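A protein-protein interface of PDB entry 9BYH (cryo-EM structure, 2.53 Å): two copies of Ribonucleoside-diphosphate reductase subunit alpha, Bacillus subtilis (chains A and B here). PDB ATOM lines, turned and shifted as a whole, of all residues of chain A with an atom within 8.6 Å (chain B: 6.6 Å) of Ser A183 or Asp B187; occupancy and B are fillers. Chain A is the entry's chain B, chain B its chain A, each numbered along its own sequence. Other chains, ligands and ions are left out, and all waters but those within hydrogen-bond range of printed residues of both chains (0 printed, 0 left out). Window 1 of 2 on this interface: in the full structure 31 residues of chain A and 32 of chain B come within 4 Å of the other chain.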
ATOM      1  N   VAL A 175     -33.960  -4.298   5.556  1.00  0.00           N
ATOM      2  CA  VAL A 175     -32.527  -4.039   5.625  1.00  0.00           C
ATOM      3  C   VAL A 175     -32.195  -2.934   4.633  1.00  0.00           C
ATOM      4  O   VAL A 175     -32.367  -3.106   3.420  1.00  0.00           O
ATOM      5  CB  VAL A 175     -31.707  -5.305   5.335  1.00  0.00           C
ATOM      6  CG1 VAL A 175     -30.275  -5.133   5.818  1.00  0.00           C
ATOM      7  CG2 VAL A 175     -32.356  -6.514   5.985  1.00  0.00           C
ATOM      8  N   ASN A 176     -31.719  -1.804   5.146  1.00  0.00           N
ATOM      9  CA  ASN A 176     -31.306  -0.705   4.290  1.00  0.00           C
ATOM     10  C   ASN A 176     -29.920  -0.973   3.712  1.00  0.00           C
ATOM     11  O   ASN A 176     -29.151  -1.793   4.220  1.00  0.00           O
ATOM     12  CB  ASN A 176     -31.312   0.613   5.062  1.00  0.00           C
ATOM     13  CG  ASN A 176     -31.785   1.778   4.221  1.00  0.00           C
ATOM     14  OD1 ASN A 176     -31.827   1.695   2.994  1.00  0.00           O
ATOM     15  ND2 ASN A 176     -32.145   2.873   4.877  1.00  0.00           N
ATOM     16  N   SER A 178     -26.711  -0.293   3.624  1.00  0.00           N
ATOM     17  CA  SER A 178     -25.571   0.278   4.325  1.00  0.00           C
ATOM     18  C   SER A 178     -24.964  -0.786   5.227  1.00  0.00           C
ATOM     19  O   SER A 178     -25.646  -1.726   5.643  1.00  0.00           O
ATOM     20  CB  SER A 178     -25.966   1.512   5.143  1.00  0.00           C
ATOM     21  OG  SER A 178     -26.327   1.158   6.463  1.00  0.00           O
ATOM     22  N   LEU A 179     -23.670  -0.630   5.517  1.00  0.00           N
ATOM     23  CA  LEU A 179     -22.995  -1.561   6.415  1.00  0.00           C
ATOM     24  C   LEU A 179     -23.566  -1.480   7.824  1.00  0.00           C
ATOM     25  O   LEU A 179     -23.719  -2.506   8.499  1.00  0.00           O
ATOM     26  CB  LEU A 179     -21.492  -1.285   6.433  1.00  0.00           C
ATOM     27  CG  LEU A 179     -20.653  -2.265   7.257  1.00  0.00           C
ATOM     28  CD1 LEU A 179     -20.729  -3.664   6.666  1.00  0.00           C
ATOM     29  CD2 LEU A 179     -19.214  -1.796   7.357  1.00  0.00           C
ATOM     30  N   ASN A 180     -23.875  -0.269   8.291  1.00  0.00           N
ATOM     31  CA  ASN A 180     -24.494  -0.118   9.603  1.00  0.00           C
ATOM     32  C   ASN A 180     -25.837  -0.833   9.653  1.00  0.00           C
ATOM     33  O   ASN A 180     -26.137  -1.542  10.621  1.00  0.00           O
ATOM     34  CB  ASN A 180     -24.669   1.363   9.935  1.00  0.00           C
ATOM     35  CG  ASN A 180     -23.386   2.010  10.407  1.00  0.00           C
ATOM     36  OD1 ASN A 180     -22.468   1.334  10.868  1.00  0.00           O
ATOM     37  ND2 ASN A 180     -23.314   3.329  10.290  1.00  0.00           N
ATOM     38  N   ASP A 181     -26.649  -0.670   8.608  1.00  0.00           N
ATOM     39  CA  ASP A 181     -27.949  -1.324   8.567  1.00  0.00           C
ATOM     40  C   ASP A 181     -27.810  -2.836   8.447  1.00  0.00           C
ATOM     41  O   ASP A 181     -28.594  -3.580   9.039  1.00  0.00           O
ATOM     42  CB  ASP A 181     -28.777  -0.761   7.414  1.00  0.00           C
ATOM     43  CG  ASP A 181     -29.201   0.674   7.653  1.00  0.00           C
ATOM     44  OD1 ASP A 181     -30.048   0.903   8.540  1.00  0.00           O
ATOM     45  OD2 ASP A 181     -28.690   1.573   6.953  1.00  0.00           O
ATOM     46  N   ILE A 182     -26.818  -3.309   7.691  1.00  0.00           N
ATOM     47  CA  ILE A 182     -26.600  -4.750   7.565  1.00  0.00           C
ATOM     48  C   ILE A 182     -26.195  -5.349   8.907  1.00  0.00           C
ATOM     49  O   ILE A 182     -26.703  -6.400   9.319  1.00  0.00           O
ATOM     50  CB  ILE A 182     -25.551  -5.037   6.476  1.00  0.00           C
ATOM     51  CG1 ILE A 182     -26.181  -4.926   5.088  1.00  0.00           C
ATOM     52  CG2 ILE A 182     -24.934  -6.415   6.669  1.00  0.00           C
ATOM     53  CD1 ILE A 182     -25.175  -4.862   3.971  1.00  0.00           C
ATOM     54  N   SER A 183     -25.272  -4.689   9.610  1.00  0.00           N
ATOM     55  CA  SER A 183     -24.848  -5.177  10.918  1.00  0.00           C
ATOM     56  C   SER A 183     -25.995  -5.137  11.920  1.00  0.00           C
ATOM     57  O   SER A 183     -26.157  -6.064  12.724  1.00  0.00           O
ATOM     58  CB  SER A 183     -23.660  -4.360  11.421  1.00  0.00           C
ATOM     59  OG  SER A 183     -23.991  -2.986  11.509  1.00  0.00           O
ATOM     60  N   ARG A 184     -26.804  -4.076  11.886  1.00  0.00           N
ATOM     61  CA  ARG A 184     -27.961  -4.009  12.770  1.00  0.00           C
ATOM     62  C   ARG A 184     -28.967  -5.104  12.441  1.00  0.00           C
ATOM     63  O   ARG A 184     -29.589  -5.670  13.343  1.00  0.00           O
ATOM     64  CB  ARG A 184     -28.616  -2.634  12.682  1.00  0.00           C
ATOM     65  CG  ARG A 184     -29.653  -2.390  13.762  1.00  0.00           C
ATOM     66  CD  ARG A 184     -29.062  -2.591  15.144  1.00  0.00           C
ATOM     67  NE  ARG A 184     -28.349  -1.406  15.604  1.00  0.00           N
ATOM     68  CZ  ARG A 184     -27.852  -1.257  16.824  1.00  0.00           C
ATOM     69  NH1 ARG A 184     -27.955  -2.214  17.733  1.00  0.00           N
ATOM     70  NH2 ARG A 184     -27.237  -0.122  17.140  1.00  0.00           N
ATOM     71  N   ALA A 185     -29.148  -5.408  11.155  1.00  0.00           N
ATOM     72  CA  ALA A 185     -30.048  -6.487  10.767  1.00  0.00           C
ATOM     73  C   ALA A 185     -29.543  -7.829  11.273  1.00  0.00           C
ATOM     74  O   ALA A 185     -30.330  -8.657  11.741  1.00  0.00           O
ATOM     75  CB  ALA A 185     -30.214  -6.515   9.249  1.00  0.00           C
ATOM     76  N   ILE A 186     -28.233  -8.064  11.185  1.00  0.00           N
ATOM     77  CA  ILE A 186     -27.661  -9.298  11.721  1.00  0.00           C
ATOM     78  C   ILE A 186     -27.890  -9.379  13.226  1.00  0.00           C
ATOM     79  O   ILE A 186     -28.286 -10.426  13.758  1.00  0.00           O
ATOM     80  CB  ILE A 186     -26.164  -9.388  11.371  1.00  0.00           C
ATOM     81  CG1 ILE A 186     -25.973  -9.527   9.861  1.00  0.00           C
ATOM     82  CG2 ILE A 186     -25.511 -10.551  12.098  1.00  0.00           C
ATOM     83  CD1 ILE A 186     -24.607  -9.093   9.386  1.00  0.00           C
ATOM     84  N   ASP A 187     -27.651  -8.272  13.933  1.00  0.00           N
ATOM     85  CA  ASP A 187     -27.851  -8.248  15.379  1.00  0.00           C
ATOM     86  C   ASP A 187     -29.305  -8.525  15.740  1.00  0.00           C
ATOM     87  O   ASP A 187     -29.592  -9.325  16.636  1.00  0.00           O
ATOM     88  CB  ASP A 187     -27.403  -6.898  15.941  1.00  0.00           C
ATOM     89  CG  ASP A 187     -27.943  -6.636  17.333  1.00  0.00           C
ATOM     90  OD1 ASP A 187     -27.746  -7.491  18.223  1.00  0.00           O
ATOM     91  OD2 ASP A 187     -28.565  -5.574  17.540  1.00  0.00           O
ATOM     92  N   ILE A 188     -30.239  -7.873  15.045  1.00  0.00           N
ATOM     93  CA  ILE A 188     -31.657  -8.042  15.345  1.00  0.00           C
ATOM     94  C   ILE A 188     -32.114  -9.453  14.999  1.00  0.00           C
ATOM     95  O   ILE A 188     -32.946 -10.038  15.700  1.00  0.00           O
ATOM     96  CB  ILE A 188     -32.488  -6.973  14.610  1.00  0.00           C
ATOM     97  CG1 ILE A 188     -32.142  -5.578  15.129  1.00  0.00           C
ATOM     98  CG2 ILE A 188     -33.970  -7.220  14.796  1.00  0.00           C
ATOM     99  CD1 ILE A 188     -32.723  -4.458  14.298  1.00  0.00           C
ATOM    100  N   SER A 189     -31.581 -10.024  13.917  1.00  0.00           N
ATOM    101  CA  SER A 189     -31.907 -11.403  13.574  1.00  0.00           C
ATOM    102  C   SER A 189     -31.443 -12.361  14.659  1.00  0.00           C
ATOM    103  O   SER A 189     -32.183 -13.270  15.050  1.00  0.00           O
ATOM    104  CB  SER A 189     -31.279 -11.770  12.230  1.00  0.00           C
ATOM    105  OG  SER A 189     -31.685 -10.869  11.217  1.00  0.00           O
ATOM    106  N   MET A 190     -30.220 -12.169  15.164  1.00  0.00           N
ATOM    107  CA  MET A 190     -29.746 -13.010  16.259  1.00  0.00           C
ATOM    108  C   MET A 190     -30.597 -12.824  17.509  1.00  0.00           C
ATOM    109  O   MET A 190     -30.914 -13.796  18.203  1.00  0.00           O
ATOM    110  CB  MET A 190     -28.279 -12.716  16.567  1.00  0.00           C
ATOM    111  CG  MET A 190     -27.315 -13.139  15.477  1.00  0.00           C
ATOM    112  SD  MET A 190     -25.593 -13.041  16.000  1.00  0.00           S
ATOM    113  CE  MET A 190     -25.232 -11.321  15.667  1.00  0.00           C
ATOM    114  N   LEU A 201     -35.997 -11.261   6.297  1.00  0.00           N
ATOM    115  CA  LEU A 201     -35.294 -10.032   5.961  1.00  0.00           C
ATOM    116  C   LEU A 201     -35.458  -9.734   4.479  1.00  0.00           C
ATOM    117  O   LEU A 201     -35.232 -10.609   3.636  1.00  0.00           O
ATOM    118  CB  LEU A 201     -33.810 -10.134   6.318  1.00  0.00           C
ATOM    119  CG  LEU A 201     -33.504 -10.458   7.780  1.00  0.00           C
ATOM    120  CD1 LEU A 201     -33.045 -11.900   7.922  1.00  0.00           C
ATOM    121  CD2 LEU A 201     -32.463  -9.499   8.328  1.00  0.00           C
ATOM    122  N   LEU A 206     -30.616  -3.741  -0.617  1.00  0.00           N
ATOM    123  CA  LEU A 206     -29.169  -3.882  -0.704  1.00  0.00           C
ATOM    124  C   LEU A 206     -28.726  -3.859  -2.159  1.00  0.00           C
ATOM    125  O   LEU A 206     -29.319  -4.523  -3.014  1.00  0.00           O
ATOM    126  CB  LEU A 206     -28.727  -5.184  -0.041  1.00  0.00           C
ATOM    127  CG  LEU A 206     -29.167  -5.384   1.407  1.00  0.00           C
ATOM    128  CD1 LEU A 206     -28.787  -6.770   1.883  1.00  0.00           C
ATOM    129  CD2 LEU A 206     -28.547  -4.323   2.294  1.00  0.00           C
ATOM    130  N   VAL A 226     -24.369 -10.727   2.334  1.00  0.00           N
ATOM    131  CA  VAL A 226     -25.296 -10.509   3.438  1.00  0.00           C
ATOM    132  C   VAL A 226     -26.054 -11.788   3.750  1.00  0.00           C
ATOM    133  O   VAL A 226     -26.366 -12.067   4.912  1.00  0.00           O
ATOM    134  CB  VAL A 226     -26.256  -9.351   3.109  1.00  0.00           C
ATOM    135  CG1 VAL A 226     -26.982  -8.889   4.362  1.00  0.00           C
ATOM    136  CG2 VAL A 226     -25.496  -8.207   2.471  1.00  0.00           C
ATOM    137  N   LEU A 229     -23.754 -13.886   5.834  1.00  0.00           N
ATOM    138  CA  LEU A 229     -23.705 -13.333   7.185  1.00  0.00           C
ATOM    139  C   LEU A 229     -24.955 -13.704   7.972  1.00  0.00           C
ATOM    140  O   LEU A 229     -24.874 -14.116   9.134  1.00  0.00           O
ATOM    141  CB  LEU A 229     -23.548 -11.816   7.128  1.00  0.00           C
ATOM    142  CG  LEU A 229     -22.279 -11.249   6.502  1.00  0.00           C
ATOM    143  CD1 LEU A 229     -22.572  -9.875   5.937  1.00  0.00           C
ATOM    144  CD2 LEU A 229     -21.164 -11.191   7.527  1.00  0.00           C
ATOM    145  N   LEU A 230     -26.125 -13.564   7.346  1.00  0.00           N
ATOM    146  CA  LEU A 230     -27.377 -13.901   8.014  1.00  0.00           C
ATOM    147  C   LEU A 230     -27.468 -15.394   8.291  1.00  0.00           C
ATOM    148  O   LEU A 230     -27.990 -15.804   9.331  1.00  0.00           O
ATOM    149  CB  LEU A 230     -28.562 -13.436   7.169  1.00  0.00           C
ATOM    150  CG  LEU A 230     -28.779 -11.926   7.085  1.00  0.00           C
ATOM    151  CD1 LEU A 230     -29.776 -11.592   5.989  1.00  0.00           C
ATOM    152  CD2 LEU A 230     -29.238 -11.375   8.425  1.00  0.00           C
ATOM    153  N   ALA A 233     -25.405 -16.011  11.257  1.00  0.00           N
ATOM    154  CA  ALA A 233     -26.073 -15.450  12.427  1.00  0.00           C
ATOM    155  C   ALA A 233     -27.199 -16.355  12.910  1.00  0.00           C
ATOM    156  O   ALA A 233     -27.366 -16.565  14.117  1.00  0.00           O
ATOM    157  CB  ALA A 233     -26.606 -14.055  12.102  1.00  0.00           C
ATOM    158  N   TYR A 394     -30.448   2.957  10.298  1.00  0.00           N
ATOM    159  CA  TYR A 394     -29.529   2.765  11.414  1.00  0.00           C
ATOM    160  C   TYR A 394     -28.227   3.482  11.085  1.00  0.00           C
ATOM    161  O   TYR A 394     -27.486   3.062  10.190  1.00  0.00           O
ATOM    162  CB  TYR A 394     -29.301   1.279  11.671  1.00  0.00           C
ATOM    163  CG  TYR A 394     -30.555   0.535  12.069  1.00  0.00           C
ATOM    164  CD1 TYR A 394     -31.182   0.792  13.279  1.00  0.00           C
ATOM    165  CD2 TYR A 394     -31.115  -0.419  11.230  1.00  0.00           C
ATOM    166  CE1 TYR A 394     -32.328   0.115  13.647  1.00  0.00           C
ATOM    167  CE2 TYR A 394     -32.261  -1.100  11.589  1.00  0.00           C
ATOM    168  CZ  TYR A 394     -32.864  -0.829  12.797  1.00  0.00           C
ATOM    169  OH  TYR A 394     -34.007  -1.504  13.160  1.00  0.00           O
ATOM    170  N   THR A 395     -27.952   4.564  11.800  1.00  0.00           N
ATOM    171  CA  THR A 395     -26.826   5.431  11.508  1.00  0.00           C
ATOM    172  C   THR A 395     -25.606   5.001  12.319  1.00  0.00           C
ATOM    173  O   THR A 395     -25.597   3.952  12.970  1.00  0.00           O
ATOM    174  CB  THR A 395     -27.209   6.886  11.783  1.00  0.00           C
ATOM    175  OG1 THR A 395     -27.646   7.016  13.142  1.00  0.00           O
ATOM    176  CG2 THR A 395     -28.332   7.320  10.856  1.00  0.00           C
ATOM    177  N   ASP A 396     -24.558   5.818  12.277  1.00  0.00           N
ATOM    178  CA  ASP A 396     -23.342   5.527  13.018  1.00  0.00           C
ATOM    179  C   ASP A 396     -23.589   5.633  14.519  1.00  0.00           C
ATOM    180  O   ASP A 396     -24.608   6.158  14.975  1.00  0.00           O
ATOM    181  CB  ASP A 396     -22.220   6.483  12.611  1.00  0.00           C
ATOM    182  CG  ASP A 396     -21.811   6.323  11.162  1.00  0.00           C
ATOM    183  OD1 ASP A 396     -22.051   5.241  10.589  1.00  0.00           O
ATOM    184  OD2 ASP A 396     -21.244   7.282  10.598  1.00  0.00           O
ATOM    185  N   TYR A 397     -22.640   5.112  15.291  1.00  0.00           N
ATOM    186  CA  TYR A 397     -22.695   5.266  16.736  1.00  0.00           C
ATOM    187  C   TYR A 397     -22.610   6.743  17.103  1.00  0.00           C
ATOM    188  O   TYR A 397     -21.973   7.541  16.412  1.00  0.00           O
ATOM    189  CB  TYR A 397     -21.561   4.485  17.402  1.00  0.00           C
ATOM    190  CG  TYR A 397     -21.849   4.093  18.832  1.00  0.00           C
ATOM    191  CD1 TYR A 397     -21.592   4.969  19.877  1.00  0.00           C
ATOM    192  CD2 TYR A 397     -22.375   2.846  19.137  1.00  0.00           C
ATOM    193  CE1 TYR A 397     -21.853   4.615  21.185  1.00  0.00           C
ATOM    194  CE2 TYR A 397     -22.638   2.483  20.442  1.00  0.00           C
ATOM    195  CZ  TYR A 397     -22.375   3.371  21.461  1.00  0.00           C
ATOM    196  OH  TYR A 397     -22.637   3.015  22.763  1.00  0.00           O
ATOM    197  N   ILE B 182     -21.451  -9.529  21.424  1.00  0.00           N
ATOM    198  CA  ILE B 182     -20.933 -10.266  20.275  1.00  0.00           C
ATOM    199  C   ILE B 182     -21.371  -9.609  18.970  1.00  0.00           C
ATOM    200  O   ILE B 182     -20.570  -9.444  18.039  1.00  0.00           O
ATOM    201  CB  ILE B 182     -21.372 -11.739  20.352  1.00  0.00           C
ATOM    202  CG1 ILE B 182     -20.488 -12.494  21.344  1.00  0.00           C
ATOM    203  CG2 ILE B 182     -21.320 -12.396  18.979  1.00  0.00           C
ATOM    204  CD1 ILE B 182     -21.048 -13.817  21.763  1.00  0.00           C
ATOM    205  N   SER B 183     -22.644  -9.220  18.880  1.00  0.00           N
ATOM    206  CA  SER B 183     -23.126  -8.544  17.681  1.00  0.00           C
ATOM    207  C   SER B 183     -22.439  -7.198  17.491  1.00  0.00           C
ATOM    208  O   SER B 183     -22.088  -6.826  16.363  1.00  0.00           O
ATOM    209  CB  SER B 183     -24.642  -8.370  17.752  1.00  0.00           C
ATOM    210  OG  SER B 183     -25.007  -7.511  18.815  1.00  0.00           O
ATOM    211  N   ARG B 184     -22.233  -6.455  18.581  1.00  0.00           N
ATOM    212  CA  ARG B 184     -21.522  -5.187  18.482  1.00  0.00           C
ATOM    213  C   ARG B 184     -20.075  -5.397  18.059  1.00  0.00           C
ATOM    214  O   ARG B 184     -19.526  -4.594  17.300  1.00  0.00           O
ATOM    215  CB  ARG B 184     -21.592  -4.439  19.811  1.00  0.00           C
ATOM    216  CG  ARG B 184     -20.923  -3.079  19.787  1.00  0.00           C
ATOM    217  CD  ARG B 184     -21.466  -2.212  18.668  1.00  0.00           C
ATOM    218  NE  ARG B 184     -22.690  -1.524  19.058  1.00  0.00           N
ATOM    219  CZ  ARG B 184     -23.645  -1.161  18.213  1.00  0.00           C
ATOM    220  NH1 ARG B 184     -23.552  -1.409  16.917  1.00  0.00           N
ATOM    221  NH2 ARG B 184     -24.720  -0.533  18.681  1.00  0.00           N
ATOM    222  N   ALA B 185     -19.437  -6.463  18.545  1.00  0.00           N
ATOM    223  CA  ALA B 185     -18.074  -6.768  18.129  1.00  0.00           C
ATOM    224  C   ALA B 185     -18.014  -7.096  16.645  1.00  0.00           C
ATOM    225  O   ALA B 185     -17.095  -6.661  15.945  1.00  0.00           O
ATOM    226  CB  ALA B 185     -17.518  -7.926  18.956  1.00  0.00           C
ATOM    227  N   ILE B 186     -18.989  -7.860  16.147  1.00  0.00           N
ATOM    228  CA  ILE B 186     -19.050  -8.155  14.715  1.00  0.00           C
ATOM    229  C   ILE B 186     -19.218  -6.867  13.917  1.00  0.00           C
ATOM    230  O   ILE B 186     -18.542  -6.646  12.902  1.00  0.00           O
ATOM    231  CB  ILE B 186     -20.186  -9.152  14.423  1.00  0.00           C
ATOM    232  CG1 ILE B 186     -19.869 -10.520  15.025  1.00  0.00           C
ATOM    233  CG2 ILE B 186     -20.428  -9.270  12.926  1.00  0.00           C
ATOM    234  CD1 ILE B 186     -21.096 -11.362  15.291  1.00  0.00           C
ATOM    235  N   ASP B 187     -20.117  -5.993  14.372  1.00  0.00           N
ATOM    236  CA  ASP B 187     -20.349  -4.729  13.680  1.00  0.00           C
ATOM    237  C   ASP B 187     -19.091  -3.868  13.662  1.00  0.00           C
ATOM    238  O   ASP B 187     -18.725  -3.305  12.625  1.00  0.00           O
ATOM    239  CB  ASP B 187     -21.504  -3.978  14.341  1.00  0.00           C
ATOM    240  CG  ASP B 187     -21.481  -2.493  14.042  1.00  0.00           C
ATOM    241  OD1 ASP B 187     -21.480  -2.123  12.849  1.00  0.00           O
ATOM    242  OD2 ASP B 187     -21.461  -1.694  15.000  1.00  0.00           O
ATOM    243  N   ILE B 188     -18.417  -3.752  14.808  1.00  0.00           N
ATOM    244  CA  ILE B 188     -17.222  -2.919  14.896  1.00  0.00           C
ATOM    245  C   ILE B 188     -16.098  -3.508  14.055  1.00  0.00           C
ATOM    246  O   ILE B 188     -15.336  -2.773  13.416  1.00  0.00           O
ATOM    247  CB  ILE B 188     -16.803  -2.739  16.367  1.00  0.00           C
ATOM    248  CG1 ILE B 188     -17.874  -1.970  17.140  1.00  0.00           C
ATOM    249  CG2 ILE B 188     -15.489  -1.995  16.465  1.00  0.00           C
ATOM    250  CD1 ILE B 188     -17.614  -1.899  18.626  1.00  0.00           C
ATOM    251  N   SER B 189     -15.971  -4.837  14.039  1.00  0.00           N
ATOM    252  CA  SER B 189     -14.977  -5.475  13.185  1.00  0.00           C
ATOM    253  C   SER B 189     -15.242  -5.171  11.719  1.00  0.00           C
ATOM    254  O   SER B 189     -14.313  -4.871  10.962  1.00  0.00           O
ATOM    255  CB  SER B 189     -14.973  -6.984  13.426  1.00  0.00           C
ATOM    256  OG  SER B 189     -14.798  -7.281  14.797  1.00  0.00           O
ATOM    257  N   MET B 190     -16.509  -5.236  11.304  1.00  0.00           N
ATOM    258  CA  MET B 190     -16.856  -4.894   9.928  1.00  0.00           C
ATOM    259  C   MET B 190     -16.536  -3.437   9.620  1.00  0.00           C
ATOM    260  O   MET B 190     -15.998  -3.123   8.553  1.00  0.00           O
ATOM    261  CB  MET B 190     -18.335  -5.175   9.679  1.00  0.00           C
ATOM    262  CG  MET B 190     -18.653  -6.618   9.372  1.00  0.00           C
ATOM    263  SD  MET B 190     -20.396  -6.969   9.628  1.00  0.00           S
ATOM    264  CE  MET B 190     -20.835  -7.568   8.006  1.00  0.00           C
ATOM    265  N   GLN B 191     -16.864  -2.530  10.544  1.00  0.00           N
ATOM    266  CA  GLN B 191     -16.624  -1.110  10.310  1.00  0.00           C
ATOM    267  C   GLN B 191     -15.134  -0.803  10.229  1.00  0.00           C
ATOM    268  O   GLN B 191     -14.710   0.029   9.418  1.00  0.00           O
ATOM    269  CB  GLN B 191     -17.281  -0.273  11.406  1.00  0.00           C
ATOM    270  CG  GLN B 191     -18.787  -0.436  11.508  1.00  0.00           C
ATOM    271  CD  GLN B 191     -19.528   0.161  10.330  1.00  0.00           C
ATOM    272  OE1 GLN B 191     -19.006   1.022   9.621  1.00  0.00           O
ATOM    273  NE2 GLN B 191     -20.757  -0.293  10.117  1.00  0.00           N
ATOM    274  N   LEU B 192     -14.325  -1.453  11.065  1.00  0.00           N
ATOM    275  CA  LEU B 192     -12.891  -1.196  11.058  1.00  0.00           C
ATOM    276  C   LEU B 192     -12.196  -1.859   9.876  1.00  0.00           C
ATOM    277  O   LEU B 192     -11.213  -1.315   9.362  1.00  0.00           O
ATOM    278  CB  LEU B 192     -12.266  -1.662  12.372  1.00  0.00           C
ATOM    279  CG  LEU B 192     -12.741  -0.947  13.638  1.00  0.00           C
ATOM    280  CD1 LEU B 192     -12.279  -1.696  14.876  1.00  0.00           C
ATOM    281  CD2 LEU B 192     -12.268   0.495  13.667  1.00  0.00           C
ATOM    282  N   LEU B 230     -17.246 -14.001  13.173  1.00  0.00           N
ATOM    283  CA  LEU B 230     -16.216 -13.006  12.896  1.00  0.00           C
ATOM    284  C   LEU B 230     -15.524 -13.280  11.570  1.00  0.00           C
ATOM    285  O   LEU B 230     -15.190 -12.347  10.837  1.00  0.00           O
ATOM    286  CB  LEU B 230     -15.200 -12.972  14.036  1.00  0.00           C
ATOM    287  CG  LEU B 230     -15.689 -12.369  15.352  1.00  0.00           C
ATOM    288  CD1 LEU B 230     -14.671 -12.597  16.456  1.00  0.00           C
ATOM    289  CD2 LEU B 230     -15.987 -10.887  15.184  1.00  0.00           C
ATOM    290  N   ALA B 233     -17.780 -12.083   8.935  1.00  0.00           N
ATOM    291  CA  ALA B 233     -17.771 -10.624   8.918  1.00  0.00           C
ATOM    292  C   ALA B 233     -16.517 -10.083   8.243  1.00  0.00           C
ATOM    293  O   ALA B 233     -16.580  -9.108   7.487  1.00  0.00           O
ATOM    294  CB  ALA B 233     -17.890 -10.086  10.343  1.00  0.00           C
ATOM    295  N   ASN B 447     -17.762   4.703  14.485  1.00  0.00           N
ATOM    296  CA  ASN B 447     -18.464   3.433  14.592  1.00  0.00           C
ATOM    297  C   ASN B 447     -17.813   2.474  15.576  1.00  0.00           C
ATOM    298  O   ASN B 447     -18.317   1.359  15.757  1.00  0.00           O
ATOM    299  CB  ASN B 447     -18.565   2.767  13.214  1.00  0.00           C
ATOM    300  CG  ASN B 447     -19.812   3.178  12.462  1.00  0.00           C
ATOM    301  OD1 ASN B 447     -20.852   3.446  13.060  1.00  0.00           O
ATOM    302  ND2 ASN B 447     -19.711   3.238  11.140  1.00  0.00           N
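Ser A183 touches Asp B187, and with the chains exchanged Asp A187 touches Ser B183.
Arg A184 touches its own counterpart, Arg B184.
Met A190 touches Ser B183, but with the chains exchanged Ser A183 does not touch Met B190 (4.5 Å).
Positions printed for both chains: 182, 183, 184, 185, 186, 187, 188, 189, 190, 230 and 233.
The side-chain amide oxygen of Gln B191 is in hydrogen-bond range of the side-chain amide nitrogen of Asn B447.
The side-chain amide nitrogen (ND2) of Asn A180 sits close to the backbone NH (N) of Asp A396 (3.4 Å).
NH1 of Arg B184 lies within salt-bridge range of OD2 of Asp B187 (2.9 Å).
OG of Ser A183 sits at hydrogen-bond distance from O of Asn A180.
The guanidinium group (NH1) of Arg A184 lies within salt-bridge range of the side-chain carboxylate (OD2) of Asp A187 (3.4 Å).
The side-chain amide nitrogen (NE2) of Gln B191 lies within hydrogen-bond range of the side-chain carboxylate (OD1) of Asp B187, 3.4 Å away.
Asn A176 touches none of the printed residues of chain B.
Of the printed residues of chain B, Asp A187 touches Ser B183 (2.8 Å).
Printed residues of chain B within 4 Å of Met A190: Ser B183 (3.7 Å).
Of chain A, only Ser A183 (3.0 Å) comes within 4 Å of Asp B187.
The nearest residue of chain A that does not touch Asp B187 is Asn A180 (4.1 Å).
Of the 14 printed residues of chain B, 7 touch a printed residue of chain A.
Of the 25 printed residues of chain A, 9 touch a printed residue of chain B.
Hydrophobic or aromatic side chains of chain A within 4 Å of the printed part of chain B: Leu A179, Met A190 and Leu A229.
Among the printed residues, 12 pairs touch across the chains.
Among the printed residues, no Asp or Glu carboxylate lies within 4 Å of a Lys or Arg side-chain nitrogen of the other chain.
Among the printed residues, pairs that only touch across the chains: Leu A179 with Gln B191 (3.5 Å), Leu A229 with Met B190 (3.6 Å), Met A190 with Ser B183 (3.7 Å), Leu A179 with Met B190 (3.7 Å) and Leu A229 with Ala B233 (3.7 Å).
The guanidinium group of Arg A184 sits close to the guanidinium group of Arg B184, at 3.0 Å.
The side-chain hydroxyl (OG) of Ser B183 lies within hydrogen-bond range of the side-chain carboxylate (OD1) of Asp A187 (2.8 Å).
The side-chain hydroxyl of Ser A183 sits at hydrogen-bond distance from the side-chain carboxylate of Asp B187, at 3.0 Å.
The side-chain amide oxygen of Asn B447 is in hydrogen-bond range of the backbone NH of Tyr A397 (3.3 Å).
NE2 of Gln B191 sits at hydrogen-bond distance from OD1 of Asn A180 (2.5 Å).
ND2 of Asn B447 lies within hydrogen-bond range of OD1 of Asp A396, at 3.1 Å.
The side-chain amide nitrogen (ND2) of Asn B447 is in hydrogen-bond range of the side-chain amide oxygen (OD1) of Asn A180 (3.4 Å).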
